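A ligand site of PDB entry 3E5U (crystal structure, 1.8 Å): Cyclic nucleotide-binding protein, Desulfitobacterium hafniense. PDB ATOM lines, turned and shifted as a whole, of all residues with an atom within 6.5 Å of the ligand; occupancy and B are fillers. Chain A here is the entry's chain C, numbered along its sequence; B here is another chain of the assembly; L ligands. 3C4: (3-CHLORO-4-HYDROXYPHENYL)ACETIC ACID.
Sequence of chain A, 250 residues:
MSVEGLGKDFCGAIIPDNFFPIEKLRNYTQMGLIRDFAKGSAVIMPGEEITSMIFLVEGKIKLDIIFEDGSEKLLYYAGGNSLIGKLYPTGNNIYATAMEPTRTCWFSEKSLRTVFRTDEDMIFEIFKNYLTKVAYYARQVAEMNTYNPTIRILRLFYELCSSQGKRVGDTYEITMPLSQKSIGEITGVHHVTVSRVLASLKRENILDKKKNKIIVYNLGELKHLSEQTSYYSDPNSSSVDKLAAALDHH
The side-chain hydroxyl of Thr 90 lies within hydrogen-bond range of an oxygen (O2) of the ligand. OH of the ligand is in hydrogen-bond range of OH of Tyr 76, 2.5 Å away. NZ of Lys 86 is in salt-bridge range of O1 of the ligand (2.6 Å). The side-chain amino group (NZ) of Lys 133 sits at hydrogen-bond distance from an oxygen (OH) of the ligand (2.7 Å). The side-chain amide nitrogen of Asn 92 is in hydrogen-bond range of an oxygen (O2) of the ligand (2.8 Å). An oxygen (OH) of the ligand is in hydrogen-bond range of the backbone NH (N) of Gly 85, 2.9 Å away.
Leu 63 touches the ligand. O of Leu 83 touches OH of the ligand (3.9 Å). Ile 84 touches the ligand (CA to OH, 3.4 Å). Ile 94 touches the ligand (CG1 to O1, 3.6 Å). Tyr 130 of chain A touches the ligand. Leu 131 of chain B touches the ligand. CG1 of Val 134 of chain B touches CD1 of the ligand (3.6 Å). Ala 135 of chain B touches the ligand. Hydrophobic or aromatic side chains that line the ligand: Leu 63, Tyr 76, Ile 84, Ile 94, Tyr 130 of chain A, Leu 131 of chain B, Val 134 of chain B and Ala 135 of chain B. The nearest printed residue that does not touch the ligand is Leu 75 (4.3 Å).
The side-chain hydroxyl of Thr 90 sits at hydrogen-bond distance from the backbone NH of Asn 92. The backbone NH of Leu 63 lies within hydrogen-bond range of the backbone carbonyl oxygen of Tyr 76. The backbone carbonyl oxygen (O) of Leu 83 lies within hydrogen-bond range of the side-chain amino group (NZ) of Lys 133 (2.6 Å). The side-chain amino group (NZ) of Lys 133 lies within hydrogen-bond range of the side-chain amide oxygen (OD1) of Asn 129. The side-chain amide nitrogen of Asn 92 lies within hydrogen-bond range of the backbone carbonyl oxygen of Ala 135 of chain B, 3.2 Å away. The guanidinium group of Arg 139 of chain B sits at hydrogen-bond distance from the side-chain amide oxygen of Asn 92 (2.9 Å). The backbone carbonyl oxygen of Gly 85 lies within hydrogen-bond range of the side-chain hydroxyl of Tyr 130 of chain A (2.6 Å). N of Leu 75 is in hydrogen-bond range of O of Leu 63 (2.9 Å).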
ATOM      1  N   LEU A  63      21.548 -16.923  -7.342  1.00  0.00           N
ATOM      2  CA  LEU A  63      20.191 -17.517  -7.383  1.00  0.00           C
ATOM      3  C   LEU A  63      19.155 -16.423  -7.696  1.00  0.00           C
ATOM      4  O   LEU A  63      18.976 -15.477  -6.917  1.00  0.00           O
ATOM      5  CB  LEU A  63      19.884 -18.298  -6.090  1.00  0.00           C
ATOM      6  CG  LEU A  63      18.603 -19.171  -6.048  1.00  0.00           C
ATOM      7  CD1 LEU A  63      18.737 -20.417  -5.094  1.00  0.00           C
ATOM      8  CD2 LEU A  63      17.359 -18.350  -5.712  1.00  0.00           C
ATOM      9  N   ILE A  65      15.060 -15.355  -9.440  1.00  0.00           N
ATOM     10  CA  ILE A  65      13.650 -15.703  -9.772  1.00  0.00           C
ATOM     11  C   ILE A  65      13.385 -15.240 -11.217  1.00  0.00           C
ATOM     12  O   ILE A  65      13.971 -14.244 -11.704  1.00  0.00           O
ATOM     13  CB  ILE A  65      12.669 -15.035  -8.762  1.00  0.00           C
ATOM     14  CG1 ILE A  65      11.226 -15.586  -8.953  1.00  0.00           C
ATOM     15  CG2 ILE A  65      12.823 -13.467  -8.793  1.00  0.00           C
ATOM     16  CD1 ILE A  65      10.127 -15.043  -7.860  1.00  0.00           C
ATOM     17  N   LEU A  75      17.663 -13.008  -6.332  1.00  0.00           N
ATOM     18  CA  LEU A  75      17.234 -13.233  -4.943  1.00  0.00           C
ATOM     19  C   LEU A  75      18.441 -13.199  -3.993  1.00  0.00           C
ATOM     20  O   LEU A  75      18.453 -12.397  -3.034  1.00  0.00           O
ATOM     21  CB  LEU A  75      16.448 -14.508  -4.728  1.00  0.00           C
ATOM     22  CG  LEU A  75      15.078 -14.597  -5.430  1.00  0.00           C
ATOM     23  CD1 LEU A  75      14.326 -15.919  -4.967  1.00  0.00           C
ATOM     24  CD2 LEU A  75      14.270 -13.312  -5.283  1.00  0.00           C
ATOM     25  N   TYR A  76      19.398 -14.063  -4.255  1.00  0.00           N
ATOM     26  CA  TYR A  76      20.637 -14.060  -3.476  1.00  0.00           C
ATOM     27  C   TYR A  76      21.894 -14.680  -4.106  1.00  0.00           C
ATOM     28  O   TYR A  76      21.845 -15.397  -5.097  1.00  0.00           O
ATOM     29  CB  TYR A  76      20.365 -14.680  -2.084  1.00  0.00           C
ATOM     30  CG  TYR A  76      20.012 -16.153  -1.955  1.00  0.00           C
ATOM     31  CD1 TYR A  76      18.747 -16.539  -1.596  1.00  0.00           C
ATOM     32  CD2 TYR A  76      20.960 -17.152  -2.206  1.00  0.00           C
ATOM     33  CE1 TYR A  76      18.400 -17.865  -1.443  1.00  0.00           C
ATOM     34  CE2 TYR A  76      20.658 -18.469  -2.069  1.00  0.00           C
ATOM     35  CZ  TYR A  76      19.376 -18.856  -1.648  1.00  0.00           C
ATOM     36  OH  TYR A  76      19.129 -20.226  -1.477  1.00  0.00           O
ATOM     37  N   LEU A  83      23.004 -22.751   2.284  1.00  0.00           N
ATOM     38  CA  LEU A  83      21.925 -23.733   2.106  1.00  0.00           C
ATOM     39  C   LEU A  83      20.815 -23.133   1.227  1.00  0.00           C
ATOM     40  O   LEU A  83      20.233 -22.053   1.533  1.00  0.00           O
ATOM     41  CB  LEU A  83      21.342 -24.113   3.450  1.00  0.00           C
ATOM     42  CG  LEU A  83      20.413 -25.353   3.412  1.00  0.00           C
ATOM     43  CD1 LEU A  83      21.096 -26.685   3.006  1.00  0.00           C
ATOM     44  CD2 LEU A  83      19.688 -25.486   4.779  1.00  0.00           C
ATOM     45  N   ILE A  84      20.465 -23.839   0.159  1.00  0.00           N
ATOM     46  CA  ILE A  84      19.286 -23.510  -0.570  1.00  0.00           C
ATOM     47  C   ILE A  84      18.110 -24.368  -0.063  1.00  0.00           C
ATOM     48  O   ILE A  84      18.148 -25.576  -0.160  1.00  0.00           O
ATOM     49  CB  ILE A  84      19.458 -23.679  -2.063  1.00  0.00           C
ATOM     50  CG1 ILE A  84      20.693 -22.944  -2.583  1.00  0.00           C
ATOM     51  CG2 ILE A  84      18.140 -23.238  -2.784  1.00  0.00           C
ATOM     52  CD1 ILE A  84      21.072 -23.386  -4.056  1.00  0.00           C
ATOM     53  N   GLY A  85      17.031 -23.714   0.430  1.00  0.00           N
ATOM     54  CA  GLY A  85      16.025 -24.348   1.244  1.00  0.00           C
ATOM     55  C   GLY A  85      14.800 -24.915   0.540  1.00  0.00           C
ATOM     56  O   GLY A  85      13.720 -24.977   1.153  1.00  0.00           O
ATOM     57  N   LYS A  86      14.983 -25.313  -0.732  1.00  0.00           N
ATOM     58  CA  LYS A  86      13.892 -25.621  -1.670  1.00  0.00           C
ATOM     59  C   LYS A  86      13.463 -27.095  -1.593  1.00  0.00           C
ATOM     60  O   LYS A  86      13.451 -27.775  -2.571  1.00  0.00           O
ATOM     61  CB  LYS A  86      14.209 -25.164  -3.085  1.00  0.00           C
ATOM     62  CG  LYS A  86      14.233 -23.615  -3.218  1.00  0.00           C
ATOM     63  CD  LYS A  86      14.701 -23.180  -4.605  1.00  0.00           C
ATOM     64  CE  LYS A  86      13.828 -23.696  -5.712  1.00  0.00           C
ATOM     65  NZ  LYS A  86      12.335 -23.465  -5.573  1.00  0.00           N
ATOM     66  N   TYR A  88      10.459 -28.244  -0.863  1.00  0.00           N
ATOM     67  CA  TYR A  88       9.104 -28.438  -1.396  1.00  0.00           C
ATOM     68  C   TYR A  88       8.826 -27.434  -2.526  1.00  0.00           C
ATOM     69  O   TYR A  88       9.525 -26.392  -2.581  1.00  0.00           O
ATOM     70  CB  TYR A  88       8.047 -28.360  -0.267  1.00  0.00           C
ATOM     71  CG  TYR A  88       8.406 -29.213   0.897  1.00  0.00           C
ATOM     72  CD1 TYR A  88       8.144 -30.587   0.921  1.00  0.00           C
ATOM     73  CD2 TYR A  88       9.023 -28.677   2.015  1.00  0.00           C
ATOM     74  CE1 TYR A  88       8.507 -31.387   2.018  1.00  0.00           C
ATOM     75  CE2 TYR A  88       9.360 -29.474   3.126  1.00  0.00           C
ATOM     76  CZ  TYR A  88       9.075 -30.835   3.117  1.00  0.00           C
ATOM     77  OH  TYR A  88       9.439 -31.661   4.178  1.00  0.00           O
ATOM     78  N   THR A  90       7.435 -24.380  -4.499  1.00  0.00           N
ATOM     79  CA  THR A  90       6.970 -23.070  -4.005  1.00  0.00           C
ATOM     80  C   THR A  90       6.073 -22.292  -5.027  1.00  0.00           C
ATOM     81  O   THR A  90       5.576 -21.217  -4.709  1.00  0.00           O
ATOM     82  CB  THR A  90       8.145 -22.147  -3.645  1.00  0.00           C
ATOM     83  OG1 THR A  90       8.794 -21.755  -4.851  1.00  0.00           O
ATOM     84  CG2 THR A  90       9.158 -22.818  -2.649  1.00  0.00           C
ATOM     85  N   GLY A  91       6.023 -22.759  -6.259  1.00  0.00           N
ATOM     86  CA  GLY A  91       5.415 -21.982  -7.351  1.00  0.00           C
ATOM     87  C   GLY A  91       6.200 -20.821  -7.955  1.00  0.00           C
ATOM     88  O   GLY A  91       5.698 -20.161  -8.890  1.00  0.00           O
ATOM     89  N   ASN A  92       7.375 -20.510  -7.414  1.00  0.00           N
ATOM     90  CA  ASN A  92       8.331 -19.664  -8.057  1.00  0.00           C
ATOM     91  C   ASN A  92       9.227 -20.487  -9.009  1.00  0.00           C
ATOM     92  O   ASN A  92       9.696 -21.554  -8.637  1.00  0.00           O
ATOM     93  CB  ASN A  92       9.178 -18.954  -7.029  1.00  0.00           C
ATOM     94  CG  ASN A  92       8.339 -18.048  -6.165  1.00  0.00           C
ATOM     95  OD1 ASN A  92       7.358 -17.468  -6.640  1.00  0.00           O
ATOM     96  ND2 ASN A  92       8.704 -17.899  -4.905  1.00  0.00           N
ATOM     97  N   ASN A  93       9.445 -19.942 -10.213  1.00  0.00           N
ATOM     98  CA  ASN A  93      10.484 -20.378 -11.148  1.00  0.00           C
ATOM     99  C   ASN A  93      11.868 -19.832 -10.720  1.00  0.00           C
ATOM    100  O   ASN A  93      12.121 -18.641 -10.670  1.00  0.00           O
ATOM    101  CB  ASN A  93      10.143 -19.950 -12.565  1.00  0.00           C
ATOM    102  CG  ASN A  93      11.091 -20.553 -13.630  1.00  0.00           C
ATOM    103  OD1 ASN A  93      12.027 -21.260 -13.323  1.00  0.00           O
ATOM    104  ND2 ASN A  93      10.811 -20.272 -14.862  1.00  0.00           N
ATOM    105  N   ILE A  94      12.747 -20.749 -10.353  1.00  0.00           N
ATOM    106  CA  ILE A  94      14.055 -20.333  -9.841  1.00  0.00           C
ATOM    107  C   ILE A  94      15.163 -20.726 -10.841  1.00  0.00           C
ATOM    108  O   ILE A  94      15.149 -21.820 -11.431  1.00  0.00           O
ATOM    109  CB  ILE A  94      14.313 -21.003  -8.504  1.00  0.00           C
ATOM    110  CG1 ILE A  94      13.376 -20.469  -7.393  1.00  0.00           C
ATOM    111  CG2 ILE A  94      15.901 -21.001  -8.183  1.00  0.00           C
ATOM    112  CD1 ILE A  94      13.270 -18.951  -7.160  1.00  0.00           C
ATOM    113  N   ASN A 129      18.653 -20.669   9.440  1.00  0.00           N
ATOM    114  CA  ASN A 129      18.849 -20.325   8.057  1.00  0.00           C
ATOM    115  C   ASN A 129      17.550 -19.805   7.405  1.00  0.00           C
ATOM    116  O   ASN A 129      17.569 -18.791   6.756  1.00  0.00           O
ATOM    117  CB  ASN A 129      19.481 -21.503   7.340  1.00  0.00           C
ATOM    118  CG  ASN A 129      19.800 -21.222   5.873  1.00  0.00           C
ATOM    119  OD1 ASN A 129      18.924 -21.381   5.047  1.00  0.00           O
ATOM    120  ND2 ASN A 129      21.035 -20.856   5.555  1.00  0.00           N
ATOM    121  N   TYR A 130      16.422 -20.487   7.604  1.00  0.00           N
ATOM    122  CA  TYR A 130      15.137 -20.041   7.098  1.00  0.00           C
ATOM    123  C   TYR A 130      14.739 -18.710   7.702  1.00  0.00           C
ATOM    124  O   TYR A 130      14.258 -17.858   6.975  1.00  0.00           O
ATOM    125  CB  TYR A 130      14.056 -21.050   7.385  1.00  0.00           C
ATOM    126  CG  TYR A 130      13.897 -22.223   6.403  1.00  0.00           C
ATOM    127  CD1 TYR A 130      13.947 -23.548   6.811  1.00  0.00           C
ATOM    128  CD2 TYR A 130      13.550 -21.993   5.084  1.00  0.00           C
ATOM    129  CE1 TYR A 130      13.738 -24.626   5.902  1.00  0.00           C
ATOM    130  CE2 TYR A 130      13.333 -23.055   4.185  1.00  0.00           C
ATOM    131  CZ  TYR A 130      13.349 -24.333   4.596  1.00  0.00           C
ATOM    132  OH  TYR A 130      13.173 -25.341   3.636  1.00  0.00           O
ATOM    133  N   LYS A 133      16.420 -15.725   6.248  1.00  0.00           N
ATOM    134  CA  LYS A 133      15.785 -15.376   4.950  1.00  0.00           C
ATOM    135  C   LYS A 133      14.440 -14.616   5.100  1.00  0.00           C
ATOM    136  O   LYS A 133      14.235 -13.581   4.501  1.00  0.00           O
ATOM    137  CB  LYS A 133      15.673 -16.664   4.099  1.00  0.00           C
ATOM    138  CG  LYS A 133      16.964 -17.280   3.684  1.00  0.00           C
ATOM    139  CD  LYS A 133      16.832 -18.634   3.032  1.00  0.00           C
ATOM    140  CE  LYS A 133      18.194 -19.264   2.685  1.00  0.00           C
ATOM    141  NZ  LYS A 133      18.078 -20.664   2.197  1.00  0.00           N
ATOM    142  N   CYS B  11       4.078 -25.033  -1.035  1.00  0.00           N
ATOM    143  CA  CYS B  11       4.525 -23.881  -0.258  1.00  0.00           C
ATOM    144  C   CYS B  11       4.459 -22.548  -1.031  1.00  0.00           C
ATOM    145  O   CYS B  11       5.330 -21.703  -0.939  1.00  0.00           O
ATOM    146  CB  CYS B  11       5.933 -24.129   0.232  1.00  0.00           C
ATOM    147  SG  CYS B  11       6.100 -25.563   1.406  1.00  0.00           S
ATOM    148  N   TYR B 130       8.191 -22.031   7.087  1.00  0.00           N
ATOM    149  CA  TYR B 130       9.286 -21.096   6.799  1.00  0.00           C
ATOM    150  C   TYR B 130       9.388 -20.888   5.280  1.00  0.00           C
ATOM    151  O   TYR B 130       9.542 -19.782   4.817  1.00  0.00           O
ATOM    152  CB  TYR B 130      10.581 -21.621   7.292  1.00  0.00           C
ATOM    153  CG  TYR B 130      10.897 -21.289   8.744  1.00  0.00           C
ATOM    154  CD1 TYR B 130      11.175 -22.303   9.652  1.00  0.00           C
ATOM    155  CD2 TYR B 130      10.927 -19.918   9.213  1.00  0.00           C
ATOM    156  CE1 TYR B 130      11.529 -21.971  11.005  1.00  0.00           C
ATOM    157  CE2 TYR B 130      11.300 -19.594  10.515  1.00  0.00           C
ATOM    158  CZ  TYR B 130      11.587 -20.652  11.434  1.00  0.00           C
ATOM    159  OH  TYR B 130      11.902 -20.284  12.748  1.00  0.00           O
ATOM    160  N   LEU B 131       9.332 -21.976   4.544  1.00  0.00           N
ATOM    161  CA  LEU B 131       9.607 -21.940   3.102  1.00  0.00           C
ATOM    162  C   LEU B 131       8.554 -21.130   2.397  1.00  0.00           C
ATOM    163  O   LEU B 131       8.875 -20.366   1.497  1.00  0.00           O
ATOM    164  CB  LEU B 131       9.777 -23.384   2.526  1.00  0.00           C
ATOM    165  CG  LEU B 131       9.937 -23.462   0.976  1.00  0.00           C
ATOM    166  CD1 LEU B 131      11.166 -22.646   0.434  1.00  0.00           C
ATOM    167  CD2 LEU B 131      10.005 -24.950   0.570  1.00  0.00           C
ATOM    168  N   VAL B 134       9.489 -17.498   3.008  1.00  0.00           N
ATOM    169  CA  VAL B 134      10.636 -17.050   2.214  1.00  0.00           C
ATOM    170  C   VAL B 134      10.145 -16.849   0.762  1.00  0.00           C
ATOM    171  O   VAL B 134      10.421 -15.824   0.167  1.00  0.00           O
ATOM    172  CB  VAL B 134      11.826 -17.959   2.299  1.00  0.00           C
ATOM    173  CG1 VAL B 134      12.974 -17.389   1.381  1.00  0.00           C
ATOM    174  CG2 VAL B 134      12.339 -18.159   3.800  1.00  0.00           C
ATOM    175  N   ALA B 135       9.428 -17.840   0.214  1.00  0.00           N
ATOM    176  CA  ALA B 135       8.983 -17.782  -1.213  1.00  0.00           C
ATOM    177  C   ALA B 135       8.067 -16.539  -1.445  1.00  0.00           C
ATOM    178  O   ALA B 135       8.183 -15.832  -2.465  1.00  0.00           O
ATOM    179  CB  ALA B 135       8.268 -19.063  -1.572  1.00  0.00           C
ATOM    180  N   TYR B 136       7.161 -16.308  -0.487  1.00  0.00           N
ATOM    181  CA  TYR B 136       6.270 -15.138  -0.496  1.00  0.00           C
ATOM    182  C   TYR B 136       7.044 -13.790  -0.581  1.00  0.00           C
ATOM    183  O   TYR B 136       6.868 -13.024  -1.559  1.00  0.00           O
ATOM    184  CB  TYR B 136       5.185 -15.172   0.655  1.00  0.00           C
ATOM    185  CG  TYR B 136       4.309 -13.911   0.517  1.00  0.00           C
ATOM    186  CD1 TYR B 136       3.258 -13.860  -0.420  1.00  0.00           C
ATOM    187  CD2 TYR B 136       4.671 -12.747   1.165  1.00  0.00           C
ATOM    188  CE1 TYR B 136       2.519 -12.699  -0.635  1.00  0.00           C
ATOM    189  CE2 TYR B 136       3.969 -11.533   0.922  1.00  0.00           C
ATOM    190  CZ  TYR B 136       2.923 -11.519   0.002  1.00  0.00           C
ATOM    191  OH  TYR B 136       2.202 -10.369  -0.205  1.00  0.00           O
ATOM    192  N   ALA B 138      10.344 -13.027  -0.793  1.00  0.00           N
ATOM    193  CA  ALA B 138      11.390 -12.990  -1.902  1.00  0.00           C
ATOM    194  C   ALA B 138      10.737 -12.658  -3.244  1.00  0.00           C
ATOM    195  O   ALA B 138      11.167 -11.704  -3.854  1.00  0.00           O
ATOM    196  CB  ALA B 138      12.207 -14.266  -1.983  1.00  0.00           C
ATOM    197  N   ARG B 139       9.666 -13.364  -3.639  1.00  0.00           N
ATOM    198  CA  ARG B 139       8.866 -12.969  -4.842  1.00  0.00           C
ATOM    199  C   ARG B 139       8.348 -11.548  -4.783  1.00  0.00           C
ATOM    200  O   ARG B 139       8.423 -10.809  -5.767  1.00  0.00           O
ATOM    201  CB  ARG B 139       7.650 -13.877  -4.980  1.00  0.00           C
ATOM    202  CG  ARG B 139       7.007 -13.924  -6.352  1.00  0.00           C
ATOM    203  CD  ARG B 139       5.739 -14.762  -6.330  1.00  0.00           C
ATOM    204  NE  ARG B 139       4.947 -14.618  -7.536  1.00  0.00           N
ATOM    205  CZ  ARG B 139       5.025 -15.331  -8.659  1.00  0.00           C
ATOM    206  NH1 ARG B 139       5.951 -16.302  -8.836  1.00  0.00           N
ATOM    207  NH2 ARG B 139       4.205 -15.001  -9.664  1.00  0.00           N
HETATM  208  O2  3C4 L   1      10.465 -19.963  -4.278  1.00  0.00           O
HETATM  209  C   3C4 L   1      11.640 -20.238  -3.857  1.00  0.00           C
HETATM  210  O1  3C4 L   1      12.230 -21.350  -4.134  1.00  0.00           O
HETATM  211  CG  3C4 L   1      12.266 -19.214  -2.913  1.00  0.00           C
HETATM  212  CA  3C4 L   1      13.531 -19.716  -2.237  1.00  0.00           C
HETATM  213  CD2 3C4 L   1      14.724 -19.712  -2.877  1.00  0.00           C
HETATM  214  CE2 3C4 L   1      15.859 -20.121  -2.396  1.00  0.00           C
HETATM  215  CZ  3C4 L   1      15.916 -20.531  -0.985  1.00  0.00           C
HETATM  216  OH  3C4 L   1      17.009 -20.939  -0.283  1.00  0.00           O
HETATM  217 CL   3C4 L   1      14.493 -21.013   1.356  1.00  0.00          CL
HETATM  218  CE1 3C4 L   1      14.606 -20.498  -0.331  1.00  0.00           C
HETATM  219  CD1 3C4 L   1      13.498 -20.099  -0.960  1.00  0.00           C
